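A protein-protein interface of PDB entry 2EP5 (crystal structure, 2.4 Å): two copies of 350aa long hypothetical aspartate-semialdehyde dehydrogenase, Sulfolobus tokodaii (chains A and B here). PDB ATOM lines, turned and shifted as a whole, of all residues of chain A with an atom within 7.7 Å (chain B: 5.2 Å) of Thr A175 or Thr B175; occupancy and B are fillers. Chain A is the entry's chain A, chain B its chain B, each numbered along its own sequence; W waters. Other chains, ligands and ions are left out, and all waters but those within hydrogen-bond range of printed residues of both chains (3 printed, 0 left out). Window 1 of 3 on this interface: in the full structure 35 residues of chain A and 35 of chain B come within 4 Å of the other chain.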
ATOM      1  N   THR A 152       5.003  18.897  13.778  1.00  0.00           N
ATOM      2  CA  THR A 152       4.620  18.554  15.140  1.00  0.00           C
ATOM      3  C   THR A 152       5.773  17.848  15.852  1.00  0.00           C
ATOM      4  O   THR A 152       6.058  18.120  17.020  1.00  0.00           O
ATOM      5  CB  THR A 152       3.391  17.634  15.152  1.00  0.00           C
ATOM      6  OG1 THR A 152       2.370  18.200  14.322  1.00  0.00           O
ATOM      7  CG2 THR A 152       2.861  17.473  16.575  1.00  0.00           C
ATOM      8  N   MET A 156       7.577  18.993  19.253  1.00  0.00           N
ATOM      9  CA  MET A 156       7.615  18.087  20.401  1.00  0.00           C
ATOM     10  C   MET A 156       9.025  17.702  20.853  1.00  0.00           C
ATOM     11  O   MET A 156       9.273  17.523  22.047  1.00  0.00           O
ATOM     12  CB  MET A 156       6.847  16.806  20.083  1.00  0.00           C
ATOM     13  CG  MET A 156       5.381  16.999  19.758  1.00  0.00           C
ATOM     14  SD  MET A 156       4.485  17.952  21.003  1.00  0.00           S
ATOM     15  CE  MET A 156       3.556  19.081  19.920  1.00  0.00           C
ATOM     16  N   ILE A 172       5.607   7.386  27.115  1.00  0.00           N
ATOM     17  CA  ILE A 172       5.278   8.739  26.690  1.00  0.00           C
ATOM     18  C   ILE A 172       3.909   8.841  26.058  1.00  0.00           C
ATOM     19  O   ILE A 172       3.683   8.286  24.984  1.00  0.00           O
ATOM     20  CB  ILE A 172       6.307   9.255  25.662  1.00  0.00           C
ATOM     21  CG1 ILE A 172       7.688   9.325  26.312  1.00  0.00           C
ATOM     22  CG2 ILE A 172       5.881  10.619  25.135  1.00  0.00           C
ATOM     23  CD1 ILE A 172       8.805   9.416  25.334  1.00  0.00           C
ATOM     24  N   ILE A 173       3.003   9.552  26.729  1.00  0.00           N
ATOM     25  CA  ILE A 173       1.659   9.768  26.214  1.00  0.00           C
ATOM     26  C   ILE A 173       1.596  11.202  25.692  1.00  0.00           C
ATOM     27  O   ILE A 173       1.898  12.153  26.420  1.00  0.00           O
ATOM     28  CB  ILE A 173       0.581   9.614  27.306  1.00  0.00           C
ATOM     29  CG1 ILE A 173       0.619   8.193  27.897  1.00  0.00           C
ATOM     30  CG2 ILE A 173      -0.794   9.926  26.711  1.00  0.00           C
ATOM     31  CD1 ILE A 173       0.229   7.092  26.918  1.00  0.00           C
ATOM     32  N   ILE A 174       1.201  11.360  24.437  1.00  0.00           N
ATOM     33  CA  ILE A 174       1.124  12.690  23.856  1.00  0.00           C
ATOM     34  C   ILE A 174      -0.176  12.989  23.117  1.00  0.00           C
ATOM     35  O   ILE A 174      -0.670  12.181  22.341  1.00  0.00           O
ATOM     36  CB  ILE A 174       2.282  12.936  22.858  1.00  0.00           C
ATOM     37  CG1 ILE A 174       3.629  12.762  23.555  1.00  0.00           C
ATOM     38  CG2 ILE A 174       2.188  14.340  22.299  1.00  0.00           C
ATOM     39  CD1 ILE A 174       4.807  12.665  22.591  1.00  0.00           C
ATOM     40  N   THR A 175      -0.729  14.161  23.388  1.00  0.00           N
ATOM     41  CA  THR A 175      -1.923  14.610  22.700  1.00  0.00           C
ATOM     42  C   THR A 175      -1.503  15.904  22.012  1.00  0.00           C
ATOM     43  O   THR A 175      -0.992  16.822  22.662  1.00  0.00           O
ATOM     44  CB  THR A 175      -3.083  14.911  23.659  1.00  0.00           C
ATOM     45  OG1 THR A 175      -3.463  13.710  24.345  1.00  0.00           O
ATOM     46  CG2 THR A 175      -4.282  15.446  22.872  1.00  0.00           C
ATOM     47  N   THR A 176      -1.685  15.966  20.701  1.00  0.00           N
ATOM     48  CA  THR A 176      -1.317  17.170  19.966  1.00  0.00           C
ATOM     49  C   THR A 176      -2.556  17.863  19.404  1.00  0.00           C
ATOM     50  O   THR A 176      -3.449  17.208  18.868  1.00  0.00           O
ATOM     51  CB  THR A 176      -0.354  16.861  18.792  1.00  0.00           C
ATOM     52  OG1 THR A 176      -1.018  16.040  17.819  1.00  0.00           O
ATOM     53  CG2 THR A 176       0.894  16.151  19.295  1.00  0.00           C
ATOM     54  N   LEU A 177      -2.614  19.185  19.557  1.00  0.00           N
ATOM     55  CA  LEU A 177      -3.722  19.972  19.030  1.00  0.00           C
ATOM     56  C   LEU A 177      -3.100  20.800  17.909  1.00  0.00           C
ATOM     57  O   LEU A 177      -2.335  21.732  18.156  1.00  0.00           O
ATOM     58  CB  LEU A 177      -4.327  20.864  20.117  1.00  0.00           C
ATOM     59  CG  LEU A 177      -5.081  20.126  21.239  1.00  0.00           C
ATOM     60  CD1 LEU A 177      -4.089  19.551  22.217  1.00  0.00           C
ATOM     61  CD2 LEU A 177      -6.006  21.087  21.978  1.00  0.00           C
ATOM     62  N   GLN A 178      -3.434  20.446  16.672  1.00  0.00           N
ATOM     63  CA  GLN A 178      -2.852  21.095  15.513  1.00  0.00           C
ATOM     64  C   GLN A 178      -3.723  22.069  14.743  1.00  0.00           C
ATOM     65  O   GLN A 178      -4.884  21.791  14.425  1.00  0.00           O
ATOM     66  CB  GLN A 178      -2.299  20.005  14.590  1.00  0.00           C
ATOM     67  CG  GLN A 178      -1.497  18.994  15.403  1.00  0.00           C
ATOM     68  CD  GLN A 178      -0.858  17.888  14.594  1.00  0.00           C
ATOM     69  OE1 GLN A 178      -0.509  16.844  15.145  1.00  0.00           O
ATOM     70  NE2 GLN A 178      -0.686  18.107  13.298  1.00  0.00           N
ATOM     71  N   GLU A 205       0.169  10.608  13.734  1.00  0.00           N
ATOM     72  CA  GLU A 205       0.591   9.941  14.961  1.00  0.00           C
ATOM     73  C   GLU A 205       1.789   9.010  14.794  1.00  0.00           C
ATOM     74  O   GLU A 205       2.682   8.995  15.630  1.00  0.00           O
ATOM     75  CB  GLU A 205      -0.613   9.214  15.582  1.00  0.00           C
ATOM     76  CG  GLU A 205      -1.714  10.206  15.933  1.00  0.00           C
ATOM     77  CD  GLU A 205      -3.084   9.587  16.116  1.00  0.00           C
ATOM     78  OE1 GLU A 205      -3.471   8.696  15.331  1.00  0.00           O
ATOM     79  OE2 GLU A 205      -3.789  10.023  17.043  1.00  0.00           O
ATOM     80  N   ILE A 208       4.988  11.118  14.142  1.00  0.00           N
ATOM     81  CA  ILE A 208       5.473  11.768  15.349  1.00  0.00           C
ATOM     82  C   ILE A 208       6.306  10.813  16.185  1.00  0.00           C
ATOM     83  O   ILE A 208       7.459  11.101  16.501  1.00  0.00           O
ATOM     84  CB  ILE A 208       4.301  12.307  16.210  1.00  0.00           C
ATOM     85  CG1 ILE A 208       3.656  13.505  15.505  1.00  0.00           C
ATOM     86  CG2 ILE A 208       4.799  12.690  17.613  1.00  0.00           C
ATOM     87  CD1 ILE A 208       2.502  14.123  16.267  1.00  0.00           C
ATOM     88  N   THR A 232       2.874   7.008  22.683  1.00  0.00           N
ATOM     89  CA  THR A 232       1.553   6.811  22.099  1.00  0.00           C
ATOM     90  C   THR A 232       0.985   8.224  21.922  1.00  0.00           C
ATOM     91  O   THR A 232       0.876   8.995  22.882  1.00  0.00           O
ATOM     92  CB  THR A 232       0.650   5.958  23.028  1.00  0.00           C
ATOM     93  OG1 THR A 232       1.140   4.613  23.052  1.00  0.00           O
ATOM     94  CG2 THR A 232      -0.787   5.944  22.534  1.00  0.00           C
ATOM     95  N   VAL A 233       0.634   8.574  20.694  1.00  0.00           N
ATOM     96  CA  VAL A 233       0.138   9.918  20.455  1.00  0.00           C
ATOM     97  C   VAL A 233      -1.219  10.003  19.797  1.00  0.00           C
ATOM     98  O   VAL A 233      -1.593   9.152  18.995  1.00  0.00           O
ATOM     99  CB  VAL A 233       1.195  10.757  19.655  1.00  0.00           C
ATOM    100  CG1 VAL A 233       2.369   9.862  19.251  1.00  0.00           C
ATOM    101  CG2 VAL A 233       0.573  11.419  18.445  1.00  0.00           C
ATOM    102  N   THR A 234      -1.953  11.042  20.170  1.00  0.00           N
ATOM    103  CA  THR A 234      -3.281  11.306  19.638  1.00  0.00           C
ATOM    104  C   THR A 234      -3.246  12.720  19.059  1.00  0.00           C
ATOM    105  O   THR A 234      -3.100  13.704  19.801  1.00  0.00           O
ATOM    106  CB  THR A 234      -4.331  11.221  20.762  1.00  0.00           C
ATOM    107  OG1 THR A 234      -4.202   9.953  21.422  1.00  0.00           O
ATOM    108  CG2 THR A 234      -5.742  11.359  20.203  1.00  0.00           C
ATOM    109  N   SER A 235      -3.356  12.820  17.737  1.00  0.00           N
ATOM    110  CA  SER A 235      -3.310  14.119  17.068  1.00  0.00           C
ATOM    111  C   SER A 235      -4.698  14.620  16.697  1.00  0.00           C
ATOM    112  O   SER A 235      -5.445  13.961  15.969  1.00  0.00           O
ATOM    113  CB  SER A 235      -2.428  14.047  15.820  1.00  0.00           C
ATOM    114  OG  SER A 235      -1.121  13.620  16.150  1.00  0.00           O
ATOM    115  N   ILE A 236      -5.018  15.813  17.187  1.00  0.00           N
ATOM    116  CA  ILE A 236      -6.318  16.413  16.972  1.00  0.00           C
ATOM    117  C   ILE A 236      -6.242  17.737  16.224  1.00  0.00           C
ATOM    118  O   ILE A 236      -5.333  18.537  16.450  1.00  0.00           O
ATOM    119  CB  ILE A 236      -7.010  16.630  18.330  1.00  0.00           C
ATOM    120  CG1 ILE A 236      -7.211  15.272  19.012  1.00  0.00           C
ATOM    121  CG2 ILE A 236      -8.327  17.352  18.147  1.00  0.00           C
ATOM    122  CD1 ILE A 236      -7.681  15.363  20.435  1.00  0.00           C
ATOM    123  N   MET A 245      -0.099  22.737  19.424  1.00  0.00           N
ATOM    124  CA  MET A 245       0.051  22.562  20.852  1.00  0.00           C
ATOM    125  C   MET A 245       0.206  21.071  21.141  1.00  0.00           C
ATOM    126  O   MET A 245      -0.323  20.224  20.413  1.00  0.00           O
ATOM    127  CB  MET A 245      -1.170  23.129  21.580  1.00  0.00           C
ATOM    128  CG  MET A 245      -1.129  22.936  23.090  1.00  0.00           C
ATOM    129  SD  MET A 245      -2.244  24.058  23.961  1.00  0.00           S
ATOM    130  CE  MET A 245      -1.550  25.635  23.480  1.00  0.00           C
ATOM    131  N   GLY A 246       0.942  20.754  22.199  1.00  0.00           N
ATOM    132  CA  GLY A 246       1.139  19.367  22.562  1.00  0.00           C
ATOM    133  C   GLY A 246       1.151  19.168  24.064  1.00  0.00           C
ATOM    134  O   GLY A 246       1.863  19.874  24.787  1.00  0.00           O
ATOM    135  N   VAL A 247       0.337  18.229  24.538  1.00  0.00           N
ATOM    136  CA  VAL A 247       0.296  17.909  25.956  1.00  0.00           C
ATOM    137  C   VAL A 247       1.134  16.649  26.086  1.00  0.00           C
ATOM    138  O   VAL A 247       0.761  15.582  25.584  1.00  0.00           O
ATOM    139  CB  VAL A 247      -1.129  17.607  26.451  1.00  0.00           C
ATOM    140  CG1 VAL A 247      -1.098  17.256  27.936  1.00  0.00           C
ATOM    141  CG2 VAL A 247      -2.016  18.805  26.213  1.00  0.00           C
ATOM    142  N   ILE A 248       2.277  16.784  26.748  1.00  0.00           N
ATOM    143  CA  ILE A 248       3.193  15.678  26.924  1.00  0.00           C
ATOM    144  C   ILE A 248       3.156  15.125  28.344  1.00  0.00           C
ATOM    145  O   ILE A 248       3.277  15.869  29.320  1.00  0.00           O
ATOM    146  CB  ILE A 248       4.637  16.123  26.557  1.00  0.00           C
ATOM    147  CG1 ILE A 248       4.654  16.627  25.104  1.00  0.00           C
ATOM    148  CG2 ILE A 248       5.630  14.960  26.743  1.00  0.00           C
ATOM    149  CD1 ILE A 248       5.990  17.196  24.649  1.00  0.00           C
ATOM    150  N   ASN A 249       2.959  13.813  28.448  1.00  0.00           N
ATOM    151  CA  ASN A 249       2.932  13.144  29.742  1.00  0.00           C
ATOM    152  C   ASN A 249       3.984  12.047  29.779  1.00  0.00           C
ATOM    153  O   ASN A 249       3.834  11.010  29.132  1.00  0.00           O
ATOM    154  CB  ASN A 249       1.563  12.524  30.028  1.00  0.00           C
ATOM    155  CG  ASN A 249       0.496  13.562  30.323  1.00  0.00           C
ATOM    156  OD1 ASN A 249      -0.094  14.139  29.411  1.00  0.00           O
ATOM    157  ND2 ASN A 249       0.254  13.813  31.603  1.00  0.00           N
ATOM    158  N   ARG A 321       4.251  16.138  33.585  1.00  0.00           N
ATOM    159  CA  ARG A 321       3.449  16.711  32.514  1.00  0.00           C
ATOM    160  C   ARG A 321       3.914  18.102  32.113  1.00  0.00           C
ATOM    161  O   ARG A 321       4.480  18.841  32.919  1.00  0.00           O
ATOM    162  CB  ARG A 321       1.971  16.794  32.901  1.00  0.00           C
ATOM    163  CG  ARG A 321       1.120  17.270  31.721  1.00  0.00           C
ATOM    164  CD  ARG A 321      -0.080  18.072  32.152  1.00  0.00           C
ATOM    165  NE  ARG A 321       0.275  19.164  33.058  1.00  0.00           N
ATOM    166  CZ  ARG A 321      -0.614  19.799  33.814  1.00  0.00           C
ATOM    167  NH1 ARG A 321      -1.891  19.453  33.756  1.00  0.00           N
ATOM    168  NH2 ARG A 321      -0.224  20.744  34.657  1.00  0.00           N
ATOM    169  N   LEU A 322       3.658  18.455  30.859  1.00  0.00           N
ATOM    170  CA  LEU A 322       4.024  19.763  30.350  1.00  0.00           C
ATOM    171  C   LEU A 322       3.296  20.046  29.045  1.00  0.00           C
ATOM    172  O   LEU A 322       2.922  19.121  28.320  1.00  0.00           O
ATOM    173  CB  LEU A 322       5.545  19.862  30.162  1.00  0.00           C
ATOM    174  CG  LEU A 322       6.289  18.983  29.157  1.00  0.00           C
ATOM    175  CD1 LEU A 322       6.083  19.513  27.743  1.00  0.00           C
ATOM    176  CD2 LEU A 322       7.766  18.998  29.486  1.00  0.00           C
ATOM    177  N   VAL A 323       3.067  21.333  28.781  1.00  0.00           N
ATOM    178  CA  VAL A 323       2.391  21.796  27.572  1.00  0.00           C
ATOM    179  C   VAL A 323       3.375  22.640  26.764  1.00  0.00           C
ATOM    180  O   VAL A 323       3.993  23.575  27.284  1.00  0.00           O
ATOM    181  CB  VAL A 323       1.141  22.662  27.905  1.00  0.00           C
ATOM    182  CG1 VAL A 323       0.506  23.178  26.621  1.00  0.00           C
ATOM    183  CG2 VAL A 323       0.116  21.831  28.698  1.00  0.00           C
ATOM    184  N   VAL A 324       3.522  22.301  25.491  1.00  0.00           N
ATOM    185  CA  VAL A 324       4.435  23.018  24.617  1.00  0.00           C
ATOM    186  C   VAL A 324       3.686  23.557  23.402  1.00  0.00           C
ATOM    187  O   VAL A 324       2.720  22.955  22.929  1.00  0.00           O
ATOM    188  CB  VAL A 324       5.575  22.101  24.149  1.00  0.00           C
ATOM    189  CG1 VAL A 324       5.002  20.935  23.352  1.00  0.00           C
ATOM    190  CG2 VAL A 324       6.578  22.890  23.317  1.00  0.00           C
ATOM    191  N   ILE B 173      -4.190   8.710  32.121  1.00  0.00           N
ATOM    192  CA  ILE B 173      -3.794  10.013  31.589  1.00  0.00           C
ATOM    193  C   ILE B 173      -4.953  10.538  30.767  1.00  0.00           C
ATOM    194  O   ILE B 173      -5.353   9.919  29.783  1.00  0.00           O
ATOM    195  CB  ILE B 173      -2.571   9.905  30.651  1.00  0.00           C
ATOM    196  CG1 ILE B 173      -1.350   9.411  31.432  1.00  0.00           C
ATOM    197  CG2 ILE B 173      -2.303  11.242  29.982  1.00  0.00           C
ATOM    198  CD1 ILE B 173      -0.994  10.270  32.644  1.00  0.00           C
ATOM    199  N   ILE B 174      -5.506  11.672  31.172  1.00  0.00           N
ATOM    200  CA  ILE B 174      -6.620  12.231  30.433  1.00  0.00           C
ATOM    201  C   ILE B 174      -6.381  13.679  30.035  1.00  0.00           C
ATOM    202  O   ILE B 174      -5.927  14.496  30.841  1.00  0.00           O
ATOM    203  CB  ILE B 174      -7.934  12.211  31.250  1.00  0.00           C
ATOM    204  CG1 ILE B 174      -8.228  10.805  31.777  1.00  0.00           C
ATOM    205  CG2 ILE B 174      -9.087  12.684  30.358  1.00  0.00           C
ATOM    206  CD1 ILE B 174      -9.352  10.756  32.813  1.00  0.00           C
ATOM    207  N   THR B 175      -6.678  13.986  28.783  1.00  0.00           N
ATOM    208  CA  THR B 175      -6.572  15.350  28.298  1.00  0.00           C
ATOM    209  C   THR B 175      -7.992  15.666  27.853  1.00  0.00           C
ATOM    210  O   THR B 175      -8.600  14.893  27.112  1.00  0.00           O
ATOM    211  CB  THR B 175      -5.599  15.485  27.098  1.00  0.00           C
ATOM    212  OG1 THR B 175      -4.250  15.286  27.546  1.00  0.00           O
ATOM    213  CG2 THR B 175      -5.710  16.876  26.480  1.00  0.00           C
ATOM    214  N   THR B 176      -8.536  16.781  28.323  1.00  0.00           N
ATOM    215  CA  THR B 176      -9.896  17.139  27.937  1.00  0.00           C
ATOM    216  C   THR B 176      -9.965  18.443  27.151  1.00  0.00           C
ATOM    217  O   THR B 176      -9.228  19.384  27.426  1.00  0.00           O
ATOM    218  CB  THR B 176     -10.822  17.248  29.181  1.00  0.00           C
ATOM    219  OG1 THR B 176     -10.406  18.348  29.997  1.00  0.00           O
ATOM    220  CG2 THR B 176     -10.742  15.963  30.019  1.00  0.00           C
ATOM    221  N   LEU B 177     -10.839  18.468  26.152  1.00  0.00           N
ATOM    222  CA  LEU B 177     -11.070  19.648  25.326  1.00  0.00           C
ATOM    223  C   LEU B 177     -12.498  20.093  25.667  1.00  0.00           C
ATOM    224  O   LEU B 177     -13.469  19.488  25.204  1.00  0.00           O
ATOM    225  CB  LEU B 177     -10.969  19.283  23.845  1.00  0.00           C
ATOM    226  CG  LEU B 177      -9.635  19.404  23.087  1.00  0.00           C
ATOM    227  CD1 LEU B 177      -8.454  18.933  23.908  1.00  0.00           C
ATOM    228  CD2 LEU B 177      -9.761  18.592  21.800  1.00  0.00           C
ATOM    229  N   VAL B 233      -4.803  14.585  34.810  1.00  0.00           N
ATOM    230  CA  VAL B 233      -5.634  15.191  33.790  1.00  0.00           C
ATOM    231  C   VAL B 233      -5.194  16.597  33.381  1.00  0.00           C
ATOM    232  O   VAL B 233      -4.706  17.382  34.192  1.00  0.00           O
ATOM    233  CB  VAL B 233      -7.104  15.216  34.283  1.00  0.00           C
ATOM    234  CG1 VAL B 233      -7.142  15.797  35.672  1.00  0.00           C
ATOM    235  CG2 VAL B 233      -7.993  16.014  33.338  1.00  0.00           C
ATOM    236  N   THR B 234      -5.354  16.893  32.099  1.00  0.00           N
ATOM    237  CA  THR B 234      -5.028  18.208  31.573  1.00  0.00           C
ATOM    238  C   THR B 234      -6.283  18.689  30.869  1.00  0.00           C
ATOM    239  O   THR B 234      -6.730  18.081  29.890  1.00  0.00           O
ATOM    240  CB  THR B 234      -3.859  18.163  30.578  1.00  0.00           C
ATOM    241  OG1 THR B 234      -2.696  17.625  31.229  1.00  0.00           O
ATOM    242  CG2 THR B 234      -3.548  19.569  30.083  1.00  0.00           C
ATOM    243  N   ILE B 236      -8.285  21.574  28.797  1.00  0.00           N
ATOM    244  CA  ILE B 236      -8.048  22.660  27.865  1.00  0.00           C
ATOM    245  C   ILE B 236      -9.333  23.252  27.307  1.00  0.00           C
ATOM    246  O   ILE B 236     -10.288  22.539  27.000  1.00  0.00           O
ATOM    247  CB  ILE B 236      -7.203  22.170  26.674  1.00  0.00           C
ATOM    248  CG1 ILE B 236      -5.893  21.571  27.181  1.00  0.00           C
ATOM    249  CG2 ILE B 236      -6.945  23.313  25.716  1.00  0.00           C
ATOM    250  CD1 ILE B 236      -5.040  20.947  26.095  1.00  0.00           C
ATOM    251  N   MET B 245     -14.743  17.026  24.977  1.00  0.00           N
ATOM    252  CA  MET B 245     -14.060  15.857  24.449  1.00  0.00           C
ATOM    253  C   MET B 245     -12.969  15.376  25.397  1.00  0.00           C
ATOM    254  O   MET B 245     -12.330  16.169  26.091  1.00  0.00           O
ATOM    255  CB  MET B 245     -13.441  16.162  23.084  1.00  0.00           C
ATOM    256  CG  MET B 245     -12.626  15.005  22.528  1.00  0.00           C
ATOM    257  SD  MET B 245     -12.237  15.158  20.781  1.00  0.00           S
ATOM    258  CE  MET B 245     -13.909  15.329  20.091  1.00  0.00           C
ATOM    259  N   GLY B 246     -12.756  14.066  25.416  1.00  0.00           N
ATOM    260  CA  GLY B 246     -11.732  13.508  26.269  1.00  0.00           C
ATOM    261  C   GLY B 246     -10.882  12.482  25.545  1.00  0.00           C
ATOM    262  O   GLY B 246     -11.398  11.666  24.778  1.00  0.00           O
ATOM    263  N   VAL B 247      -9.573  12.554  25.756  1.00  0.00           N
ATOM    264  CA  VAL B 247      -8.650  11.589  25.175  1.00  0.00           C
ATOM    265  C   VAL B 247      -8.166  10.839  26.403  1.00  0.00           C
ATOM    266  O   VAL B 247      -7.503  11.410  27.262  1.00  0.00           O
ATOM    267  CB  VAL B 247      -7.453  12.254  24.494  1.00  0.00           C
ATOM    268  CG1 VAL B 247      -6.524  11.188  23.941  1.00  0.00           C
ATOM    269  CG2 VAL B 247      -7.931  13.167  23.377  1.00  0.00           C
ATOM    270  N   ASN B 249      -6.041   7.675  28.070  1.00  0.00           N
ATOM    271  CA  ASN B 249      -4.990   6.681  27.901  1.00  0.00           C
ATOM    272  C   ASN B 249      -4.804   5.888  29.196  1.00  0.00           C
ATOM    273  O   ASN B 249      -4.336   6.416  30.210  1.00  0.00           O
ATOM    274  CB  ASN B 249      -3.651   7.333  27.522  1.00  0.00           C
ATOM    275  CG  ASN B 249      -3.653   7.928  26.113  1.00  0.00           C
ATOM    276  OD1 ASN B 249      -4.046   9.082  25.906  1.00  0.00           O
ATOM    277  ND2 ASN B 249      -3.222   7.134  25.140  1.00  0.00           N
HETATM  278  O   HOH W   1      -2.472   9.493  23.144  1.00  0.00           O
HETATM  279  O   HOH W   2      -2.753  14.931  31.271  1.00  0.00           O
HETATM  280  O   HOH W   3      -4.237  12.138  27.228  1.00  0.00           O
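The guanidinium group (NH1) of Arg A321 sits close to the side-chain hydroxyl (OG1) of Thr B234, at 3.2 Å.
N of Val A247 sits at hydrogen-bond distance from O of Thr A175, at 2.7 Å. The backbone carbonyl oxygen (O) of Thr A234 is in hydrogen-bond range of the backbone NH (N) of Thr A176 (2.8 Å). The backbone NH (N) of Leu A177 lies within hydrogen-bond range of the backbone carbonyl oxygen (O) of Met A245 (2.7 Å). The backbone carbonyl oxygen (O) of Ile B173 sits at hydrogen-bond distance from the backbone NH (N) of Asn B249, at 2.9 Å. The backbone NH of Thr B234 is in hydrogen-bond range of the backbone carbonyl oxygen of Ile B174 (2.8 Å). The backbone NH (N) of Val B247 is in hydrogen-bond range of the backbone carbonyl oxygen (O) of Thr B175, at 2.9 Å.
Ile A173 touches Asn B249 (CG2 to OD1, 3.5 Å). OG1 of Thr B175 touches OG1 of Thr A175, at 3.7 Å. Val B247 touches Thr A175. CG1 of Val B247 touches OG1 of Thr A234, 3.6 Å away. CD1 of Ile A236 touches CG2 of Val B247, at 3.7 Å. CG1 of Val A247 touches OG1 of Thr B175, at 3.7 Å. CG1 of Val A247 touches OG1 of Thr B234, at 3.7 Å. Val A247 touches Ile B236 (CG2 to CD1, 3.7 Å). Asn A249 touches Ile B173. NH1 of Arg A321 touches O of Val B233 (3.5 Å).
Printed residues of chain B within 4 Å of Thr A232: Asn B249 (3.8 Å). Of the printed residues of chain B, Arg A321 touches Val B233 (3.5 Å) and Thr B234 (2.8 Å). Thr B175 touches just these residues of chain A: Thr A175 (3.7 Å) and Val A247 (3.7 Å). The nearest residue of chain A that does not touch Thr B175 is Asn A249 (4.7 Å). The nearest printed residue of chain B that does not touch Val A247 is Ile B174 (6.3 Å).
Of the 25 printed residues of chain A, 9 touch a printed residue of chain B. Among the printed residues, no Asp or Glu carboxylate lies within 4 Å of a Lys or Arg side-chain nitrogen of the other chain.
Ile B173 touches its own counterpart, Ile A173. Ile A173 touches Asn B249, and with the chains exchanged Asn A249 touches Ile B173. Thr A175 touches Val B247, and with the chains exchanged Val A247 touches Thr B175. Leu A177 touches its own counterpart, Leu B177. Positions printed for both chains: 173, 174, 175, 176, 177, 233, 234, 236, 245, 246, 247 and 249. Of the 14 pairs that touch across the chains among the printed residues, 11 have their exchanged pair printed and touching as well.
Water W1 lies within hydrogen-bond range of the side-chain hydroxyl of Thr A234 (2.5 Å), the side-chain amide nitrogen of Asn B249 (3.2 Å), the backbone carbonyl oxygen of Ile A174 (3.3 Å) and the backbone carbonyl oxygen of Thr A232 (3.4 Å). Water W2 lies within hydrogen-bond range of the side-chain hydroxyl of Thr B234, the side-chain amide nitrogen of Asn A249 and the backbone carbonyl oxygen of Ile B174. Water W3 lies within hydrogen-bond range of OG1 of Thr B175, OD1 of Asn B249, O of Val B247 and OG1 of Thr A175.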
